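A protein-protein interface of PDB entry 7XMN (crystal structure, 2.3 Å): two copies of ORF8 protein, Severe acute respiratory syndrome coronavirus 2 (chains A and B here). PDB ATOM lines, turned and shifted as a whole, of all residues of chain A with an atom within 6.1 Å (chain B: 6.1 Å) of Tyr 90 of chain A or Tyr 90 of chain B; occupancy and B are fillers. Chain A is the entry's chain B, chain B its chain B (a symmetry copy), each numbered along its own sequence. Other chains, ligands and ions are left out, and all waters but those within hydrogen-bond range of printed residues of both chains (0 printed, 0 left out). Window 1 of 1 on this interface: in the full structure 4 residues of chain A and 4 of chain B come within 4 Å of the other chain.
The side-chain hydroxyl (OH) of Tyr 90 of chain A lies within hydrogen-bond range of the side-chain hydroxyl (OH) of Tyr 90 of chain B (2.9 Å).
OH of Tyr 27 of chain A is in hydrogen-bond range of OH of Tyr 27 of chain B (2.5 Å).
The backbone NH (N) of Tyr 90 of chain A lies within hydrogen-bond range of the backbone carbonyl oxygen (O) of His 25 of chain A, 3.0 Å away.
The backbone NH of Tyr 27 of chain A is in hydrogen-bond range of the backbone carbonyl oxygen of Ser 88 of chain A (2.6 Å).
O of Ser 88 of chain B sits at hydrogen-bond distance from N of Tyr 27 of chain B, at 2.6 Å.
O of His 25 of chain B is in hydrogen-bond range of N of Tyr 90 of chain B, 3.0 Å away.
CE2 of Tyr 90 of chain B touches CE1 of Tyr 27 of chain A, at 3.9 Å.
Tyr 27 of chain B touches Tyr 90 of chain A (CE1 to CE2, 3.9 Å).
Of the printed residues of chain B, Tyr 90 of chain A touches Tyr 27 (3.9 Å) and Tyr 90 (2.9 Å).
Tyr 90 of chain B touches just these residues of chain A: Tyr 27 (3.9 Å) and Tyr 90 (2.9 Å).
Printed residues of chain B within 4 Å of Tyr 27 of chain A: Tyr 27 (2.5 Å) and Tyr 90 (3.9 Å).
Of the printed residues of chain A, Tyr 27 of chain B touches Tyr 27 (2.5 Å) and Tyr 90 (3.9 Å).
Phe 93 of chain B touches none of the printed residues of chain A.
Glu 91 of chain B touches none of the printed residues of chain A.
The nearest printed residue of chain A that does not touch Tyr 90 of chain B is Phe 26 of chain A (6.1 Å).
The nearest printed residue of chain B that does not touch Tyr 27 of chain A is His 25 of chain B (7.1 Å).
Of the 10 printed residues of chain A, 2 touch a printed residue of chain B.
Printed residues of chain A that touch a printed residue of chain B: Tyr 27 and Tyr 90.
Hydrophobic or aromatic side chains of chain A that line the printed part of chain B: Tyr 27 and Tyr 90.
Along chain A the printed residues that touch a printed residue of chain B span positions 27 to 90.
Of the 10 printed residues of chain B, 2 touch a printed residue of chain A.
Hydrophobic or aromatic side chains of chain B within 4 Å of the printed part of chain A: Tyr 27 and Tyr 90.
Among the printed residues, no Asp or Glu carboxylate lies within 4 Å of a Lys or Arg side-chain nitrogen of the other chain.
Tyr 27 of chain B touches its own counterpart, Tyr 27 of chain A.
Tyr 27 of chain A touches Tyr 90 of chain B, and with the chains exchanged Tyr 90 of chain A touches Tyr 27 of chain B.
Tyr 90 of chain B touches its own counterpart, Tyr 90 of chain A.
10 positions are printed for both chains.
Of the 4 pairs that touch across the chains among the printed residues, 4 have their exchanged pair printed and touching as well.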
ATOM      1  N   ILE A  24     -20.224   4.788 -20.410  1.00  0.00           N
ATOM      2  CA  ILE A  24     -19.647   4.964 -21.732  1.00  0.00           C
ATOM      3  C   ILE A  24     -18.310   4.220 -21.782  1.00  0.00           C
ATOM      4  O   ILE A  24     -17.610   4.084 -20.769  1.00  0.00           O
ATOM      5  CB  ILE A  24     -19.487   6.461 -22.054  1.00  0.00           C
ATOM      6  CG1 ILE A  24     -19.212   6.688 -23.545  1.00  0.00           C
ATOM      7  CG2 ILE A  24     -18.420   7.099 -21.177  1.00  0.00           C
ATOM      8  CD1 ILE A  24     -20.465   6.670 -24.401  1.00  0.00           C
ATOM      9  N   HIS A  25     -17.975   3.700 -22.963  1.00  0.00           N
ATOM     10  CA  HIS A  25     -16.784   2.883 -23.197  1.00  0.00           C
ATOM     11  C   HIS A  25     -16.858   1.527 -22.500  1.00  0.00           C
ATOM     12  O   HIS A  25     -15.823   0.917 -22.214  1.00  0.00           O
ATOM     13  CB  HIS A  25     -15.497   3.618 -22.786  1.00  0.00           C
ATOM     14  CG  HIS A  25     -14.353   3.415 -23.734  1.00  0.00           C
ATOM     15  ND1 HIS A  25     -14.358   3.903 -25.023  1.00  0.00           N
ATOM     16  CD2 HIS A  25     -13.162   2.785 -23.576  1.00  0.00           C
ATOM     17  CE1 HIS A  25     -13.227   3.575 -25.622  1.00  0.00           C
ATOM     18  NE2 HIS A  25     -12.484   2.897 -24.767  1.00  0.00           N
ATOM     19  N   PHE A  26     -18.066   1.044 -22.215  1.00  0.00           N
ATOM     20  CA  PHE A  26     -18.307  -0.320 -21.765  1.00  0.00           C
ATOM     21  C   PHE A  26     -19.314  -0.967 -22.706  1.00  0.00           C
ATOM     22  O   PHE A  26     -20.266  -0.316 -23.145  1.00  0.00           O
ATOM     23  CB  PHE A  26     -18.854  -0.366 -20.329  1.00  0.00           C
ATOM     24  CG  PHE A  26     -17.806  -0.212 -19.258  1.00  0.00           C
ATOM     25  CD1 PHE A  26     -17.252   1.027 -18.980  1.00  0.00           C
ATOM     26  CD2 PHE A  26     -17.405  -1.302 -18.503  1.00  0.00           C
ATOM     27  CE1 PHE A  26     -16.302   1.171 -17.986  1.00  0.00           C
ATOM     28  CE2 PHE A  26     -16.457  -1.167 -17.509  1.00  0.00           C
ATOM     29  CZ  PHE A  26     -15.904   0.074 -17.250  1.00  0.00           C
ATOM     30  N   TYR A  27     -19.100  -2.242 -23.027  1.00  0.00           N
ATOM     31  CA  TYR A  27     -20.064  -2.985 -23.829  1.00  0.00           C
ATOM     32  C   TYR A  27     -21.177  -3.521 -22.940  1.00  0.00           C
ATOM     33  O   TYR A  27     -20.927  -4.011 -21.836  1.00  0.00           O
ATOM     34  CB  TYR A  27     -19.394  -4.149 -24.563  1.00  0.00           C
ATOM     35  CG  TYR A  27     -18.451  -3.757 -25.680  1.00  0.00           C
ATOM     36  CD1 TYR A  27     -18.904  -3.038 -26.779  1.00  0.00           C
ATOM     37  CD2 TYR A  27     -17.112  -4.122 -25.642  1.00  0.00           C
ATOM     38  CE1 TYR A  27     -18.044  -2.682 -27.805  1.00  0.00           C
ATOM     39  CE2 TYR A  27     -16.243  -3.773 -26.660  1.00  0.00           C
ATOM     40  CZ  TYR A  27     -16.714  -3.054 -27.740  1.00  0.00           C
ATOM     41  OH  TYR A  27     -15.849  -2.707 -28.751  1.00  0.00           O
ATOM     42  N   SER A  88     -18.864  -4.558 -19.920  1.00  0.00           N
ATOM     43  CA  SER A  88     -17.499  -5.002 -20.182  1.00  0.00           C
ATOM     44  C   SER A  88     -16.699  -3.858 -20.794  1.00  0.00           C
ATOM     45  O   SER A  88     -17.107  -3.285 -21.810  1.00  0.00           O
ATOM     46  CB  SER A  88     -17.492  -6.221 -21.105  1.00  0.00           C
ATOM     47  OG  SER A  88     -18.145  -7.325 -20.498  1.00  0.00           O
ATOM     48  N   PHE A  89     -15.559  -3.543 -20.179  1.00  0.00           N
ATOM     49  CA  PHE A  89     -14.740  -2.415 -20.609  1.00  0.00           C
ATOM     50  C   PHE A  89     -14.203  -2.643 -22.018  1.00  0.00           C
ATOM     51  O   PHE A  89     -13.740  -3.738 -22.348  1.00  0.00           O
ATOM     52  CB  PHE A  89     -13.590  -2.213 -19.620  1.00  0.00           C
ATOM     53  CG  PHE A  89     -12.820  -0.939 -19.828  1.00  0.00           C
ATOM     54  CD1 PHE A  89     -13.476   0.278 -19.913  1.00  0.00           C
ATOM     55  CD2 PHE A  89     -11.437  -0.957 -19.925  1.00  0.00           C
ATOM     56  CE1 PHE A  89     -12.767   1.452 -20.102  1.00  0.00           C
ATOM     57  CE2 PHE A  89     -10.725   0.213 -20.115  1.00  0.00           C
ATOM     58  CZ  PHE A  89     -11.392   1.420 -20.202  1.00  0.00           C
ATOM     59  N   TYR A  90     -14.264  -1.592 -22.843  1.00  0.00           N
ATOM     60  CA  TYR A  90     -13.840  -1.686 -24.241  1.00  0.00           C
ATOM     61  C   TYR A  90     -12.427  -2.250 -24.373  1.00  0.00           C
ATOM     62  O   TYR A  90     -12.175  -3.140 -25.193  1.00  0.00           O
ATOM     63  CB  TYR A  90     -13.905  -0.308 -24.902  1.00  0.00           C
ATOM     64  CG  TYR A  90     -15.247   0.081 -25.493  1.00  0.00           C
ATOM     65  CD1 TYR A  90     -16.426  -0.502 -25.053  1.00  0.00           C
ATOM     66  CD2 TYR A  90     -15.328   1.045 -26.493  1.00  0.00           C
ATOM     67  CE1 TYR A  90     -17.649  -0.136 -25.593  1.00  0.00           C
ATOM     68  CE2 TYR A  90     -16.540   1.415 -27.039  1.00  0.00           C
ATOM     69  CZ  TYR A  90     -17.698   0.820 -26.587  1.00  0.00           C
ATOM     70  OH  TYR A  90     -18.910   1.186 -27.129  1.00  0.00           O
ATOM     71  N   GLU A  91     -11.489  -1.737 -23.576  1.00  0.00           N
ATOM     72  CA  GLU A  91     -10.084  -2.101 -23.721  1.00  0.00           C
ATOM     73  C   GLU A  91      -9.713  -3.400 -23.019  1.00  0.00           C
ATOM     74  O   GLU A  91      -8.583  -3.871 -23.193  1.00  0.00           O
ATOM     75  CB  GLU A  91      -9.190  -0.976 -23.190  1.00  0.00           C
ATOM     76  CG  GLU A  91      -9.646   0.420 -23.577  1.00  0.00           C
ATOM     77  CD  GLU A  91      -9.606   0.648 -25.076  1.00  0.00           C
ATOM     78  OE1 GLU A  91      -8.717   0.073 -25.738  1.00  0.00           O
ATOM     79  OE2 GLU A  91     -10.461   1.398 -25.591  1.00  0.00           O
ATOM     80  N   ASP A  92     -10.617  -3.991 -22.240  1.00  0.00           N
ATOM     81  CA  ASP A  92     -10.269  -5.171 -21.448  1.00  0.00           C
ATOM     82  C   ASP A  92     -11.561  -5.838 -20.998  1.00  0.00           C
ATOM     83  O   ASP A  92     -12.246  -5.323 -20.108  1.00  0.00           O
ATOM     84  CB  ASP A  92      -9.400  -4.772 -20.255  1.00  0.00           C
ATOM     85  CG  ASP A  92      -8.945  -5.961 -19.430  1.00  0.00           C
ATOM     86  OD1 ASP A  92      -9.266  -7.112 -19.792  1.00  0.00           O
ATOM     87  OD2 ASP A  92      -8.260  -5.739 -18.408  1.00  0.00           O
ATOM     88  N   PHE A  93     -11.886  -6.987 -21.597  1.00  0.00           N
ATOM     89  CA  PHE A  93     -13.109  -7.692 -21.235  1.00  0.00           C
ATOM     90  C   PHE A  93     -13.043  -8.314 -19.845  1.00  0.00           C
ATOM     91  O   PHE A  93     -14.079  -8.755 -19.335  1.00  0.00           O
ATOM     92  CB  PHE A  93     -13.434  -8.760 -22.287  1.00  0.00           C
ATOM     93  CG  PHE A  93     -12.637 -10.032 -22.144  1.00  0.00           C
ATOM     94  CD1 PHE A  93     -11.297 -10.073 -22.492  1.00  0.00           C
ATOM     95  CD2 PHE A  93     -13.238 -11.192 -21.683  1.00  0.00           C
ATOM     96  CE1 PHE A  93     -10.566 -11.245 -22.369  1.00  0.00           C
ATOM     97  CE2 PHE A  93     -12.513 -12.366 -21.558  1.00  0.00           C
ATOM     98  CZ  PHE A  93     -11.176 -12.392 -21.902  1.00  0.00           C
ATOM     99  N   ILE B  24     -27.119   3.305 -32.230  1.00  0.00           N
ATOM    100  CA  ILE B  24     -26.605   2.206 -31.429  1.00  0.00           C
ATOM    101  C   ILE B  24     -25.893   1.219 -32.357  1.00  0.00           C
ATOM    102  O   ILE B  24     -26.252   1.067 -33.533  1.00  0.00           O
ATOM    103  CB  ILE B  24     -27.744   1.537 -30.639  1.00  0.00           C
ATOM    104  CG1 ILE B  24     -27.201   0.619 -29.539  1.00  0.00           C
ATOM    105  CG2 ILE B  24     -28.699   0.804 -31.570  1.00  0.00           C
ATOM    106  CD1 ILE B  24     -26.802   1.358 -28.275  1.00  0.00           C
ATOM    107  N   HIS B  25     -24.849   0.574 -31.833  1.00  0.00           N
ATOM    108  CA  HIS B  25     -23.988  -0.343 -32.580  1.00  0.00           C
ATOM    109  C   HIS B  25     -23.152   0.370 -33.640  1.00  0.00           C
ATOM    110  O   HIS B  25     -22.731  -0.251 -34.621  1.00  0.00           O
ATOM    111  CB  HIS B  25     -24.791  -1.487 -33.221  1.00  0.00           C
ATOM    112  CG  HIS B  25     -24.113  -2.823 -33.142  1.00  0.00           C
ATOM    113  ND1 HIS B  25     -23.904  -3.483 -31.950  1.00  0.00           N
ATOM    114  CD2 HIS B  25     -23.608  -3.627 -34.110  1.00  0.00           C
ATOM    115  CE1 HIS B  25     -23.291  -4.630 -32.184  1.00  0.00           C
ATOM    116  NE2 HIS B  25     -23.099  -4.741 -33.486  1.00  0.00           N
ATOM    117  N   PHE B  26     -22.908   1.667 -33.464  1.00  0.00           N
ATOM    118  CA  PHE B  26     -21.950   2.425 -34.257  1.00  0.00           C
ATOM    119  C   PHE B  26     -20.954   3.081 -33.311  1.00  0.00           C
ATOM    120  O   PHE B  26     -21.334   3.556 -32.237  1.00  0.00           O
ATOM    121  CB  PHE B  26     -22.632   3.509 -35.106  1.00  0.00           C
ATOM    122  CG  PHE B  26     -23.262   3.001 -36.377  1.00  0.00           C
ATOM    123  CD1 PHE B  26     -24.459   2.307 -36.347  1.00  0.00           C
ATOM    124  CD2 PHE B  26     -22.672   3.255 -37.605  1.00  0.00           C
ATOM    125  CE1 PHE B  26     -25.045   1.855 -37.515  1.00  0.00           C
ATOM    126  CE2 PHE B  26     -23.250   2.806 -38.775  1.00  0.00           C
ATOM    127  CZ  PHE B  26     -24.440   2.105 -38.731  1.00  0.00           C
ATOM    128  N   TYR B  27     -19.681   3.099 -33.700  1.00  0.00           N
ATOM    129  CA  TYR B  27     -18.669   3.802 -32.920  1.00  0.00           C
ATOM    130  C   TYR B  27     -18.673   5.282 -33.276  1.00  0.00           C
ATOM    131  O   TYR B  27     -18.781   5.652 -34.448  1.00  0.00           O
ATOM    132  CB  TYR B  27     -17.274   3.222 -33.172  1.00  0.00           C
ATOM    133  CG  TYR B  27     -17.039   1.833 -32.617  1.00  0.00           C
ATOM    134  CD1 TYR B  27     -17.137   1.581 -31.255  1.00  0.00           C
ATOM    135  CD2 TYR B  27     -16.699   0.781 -33.456  1.00  0.00           C
ATOM    136  CE1 TYR B  27     -16.916   0.312 -30.745  1.00  0.00           C
ATOM    137  CE2 TYR B  27     -16.476  -0.491 -32.959  1.00  0.00           C
ATOM    138  CZ  TYR B  27     -16.585  -0.720 -31.602  1.00  0.00           C
ATOM    139  OH  TYR B  27     -16.364  -1.985 -31.110  1.00  0.00           O
ATOM    140  N   SER B  88     -19.185   4.798 -37.156  1.00  0.00           N
ATOM    141  CA  SER B  88     -18.629   3.619 -37.811  1.00  0.00           C
ATOM    142  C   SER B  88     -19.300   2.365 -37.260  1.00  0.00           C
ATOM    143  O   SER B  88     -19.311   2.146 -36.044  1.00  0.00           O
ATOM    144  CB  SER B  88     -17.115   3.552 -37.614  1.00  0.00           C
ATOM    145  OG  SER B  88     -16.472   4.664 -38.216  1.00  0.00           O
ATOM    146  N   PHE B  89     -19.842   1.545 -38.161  1.00  0.00           N
ATOM    147  CA  PHE B  89     -20.587   0.355 -37.765  1.00  0.00           C
ATOM    148  C   PHE B  89     -19.681  -0.637 -37.046  1.00  0.00           C
ATOM    149  O   PHE B  89     -18.552  -0.887 -37.476  1.00  0.00           O
ATOM    150  CB  PHE B  89     -21.216  -0.289 -39.004  1.00  0.00           C
ATOM    151  CG  PHE B  89     -22.199  -1.382 -38.694  1.00  0.00           C
ATOM    152  CD1 PHE B  89     -23.235  -1.169 -37.801  1.00  0.00           C
ATOM    153  CD2 PHE B  89     -22.094  -2.621 -39.307  1.00  0.00           C
ATOM    154  CE1 PHE B  89     -24.143  -2.175 -37.517  1.00  0.00           C
ATOM    155  CE2 PHE B  89     -22.998  -3.629 -39.026  1.00  0.00           C
ATOM    156  CZ  PHE B  89     -24.025  -3.405 -38.130  1.00  0.00           C
ATOM    157  N   TYR B  90     -20.191  -1.205 -35.948  1.00  0.00           N
ATOM    158  CA  TYR B  90     -19.410  -2.130 -35.126  1.00  0.00           C
ATOM    159  C   TYR B  90     -18.811  -3.265 -35.953  1.00  0.00           C
ATOM    160  O   TYR B  90     -17.626  -3.589 -35.819  1.00  0.00           O
ATOM    161  CB  TYR B  90     -20.286  -2.713 -34.015  1.00  0.00           C
ATOM    162  CG  TYR B  90     -20.375  -1.893 -32.741  1.00  0.00           C
ATOM    163  CD1 TYR B  90     -20.118  -0.529 -32.740  1.00  0.00           C
ATOM    164  CD2 TYR B  90     -20.725  -2.493 -31.536  1.00  0.00           C
ATOM    165  CE1 TYR B  90     -20.208   0.214 -31.574  1.00  0.00           C
ATOM    166  CE2 TYR B  90     -20.814  -1.762 -30.369  1.00  0.00           C
ATOM    167  CZ  TYR B  90     -20.553  -0.410 -30.392  1.00  0.00           C
ATOM    168  OH  TYR B  90     -20.642   0.323 -29.229  1.00  0.00           O
ATOM    169  N   GLU B  91     -19.621  -3.886 -36.812  1.00  0.00           N
ATOM    170  CA  GLU B  91     -19.191  -5.073 -37.542  1.00  0.00           C
ATOM    171  C   GLU B  91     -18.395  -4.760 -38.802  1.00  0.00           C
ATOM    172  O   GLU B  91     -17.866  -5.692 -39.419  1.00  0.00           O
ATOM    173  CB  GLU B  91     -20.404  -5.927 -37.921  1.00  0.00           C
ATOM    174  CG  GLU B  91     -21.443  -6.062 -36.820  1.00  0.00           C
ATOM    175  CD  GLU B  91     -20.903  -6.779 -35.599  1.00  0.00           C
ATOM    176  OE1 GLU B  91     -20.051  -7.675 -35.767  1.00  0.00           O
ATOM    177  OE2 GLU B  91     -21.329  -6.448 -34.472  1.00  0.00           O
ATOM    178  N   ASP B  92     -18.291  -3.494 -39.199  1.00  0.00           N
ATOM    179  CA  ASP B  92     -17.643  -3.156 -40.466  1.00  0.00           C
ATOM    180  C   ASP B  92     -17.322  -1.667 -40.452  1.00  0.00           C
ATOM    181  O   ASP B  92     -18.229  -0.838 -40.582  1.00  0.00           O
ATOM    182  CB  ASP B  92     -18.550  -3.521 -41.640  1.00  0.00           C
ATOM    183  CG  ASP B  92     -17.907  -3.260 -42.990  1.00  0.00           C
ATOM    184  OD1 ASP B  92     -16.738  -2.826 -43.033  1.00  0.00           O
ATOM    185  OD2 ASP B  92     -18.582  -3.491 -44.017  1.00  0.00           O
ATOM    186  N   PHE B  93     -16.037  -1.330 -40.312  1.00  0.00           N
ATOM    187  CA  PHE B  93     -15.639   0.072 -40.280  1.00  0.00           C
ATOM    188  C   PHE B  93     -15.778   0.757 -41.635  1.00  0.00           C
ATOM    189  O   PHE B  93     -15.677   1.987 -41.698  1.00  0.00           O
ATOM    190  CB  PHE B  93     -14.202   0.200 -39.759  1.00  0.00           C
ATOM    191  CG  PHE B  93     -13.141  -0.097 -40.788  1.00  0.00           C
ATOM    192  CD1 PHE B  93     -12.894  -1.397 -41.198  1.00  0.00           C
ATOM    193  CD2 PHE B  93     -12.376   0.924 -41.327  1.00  0.00           C
ATOM    194  CE1 PHE B  93     -11.913  -1.671 -42.138  1.00  0.00           C
ATOM    195  CE2 PHE B  93     -11.394   0.656 -42.267  1.00  0.00           C
ATOM    196  CZ  PHE B  93     -11.162  -0.644 -42.672  1.00  0.00           C
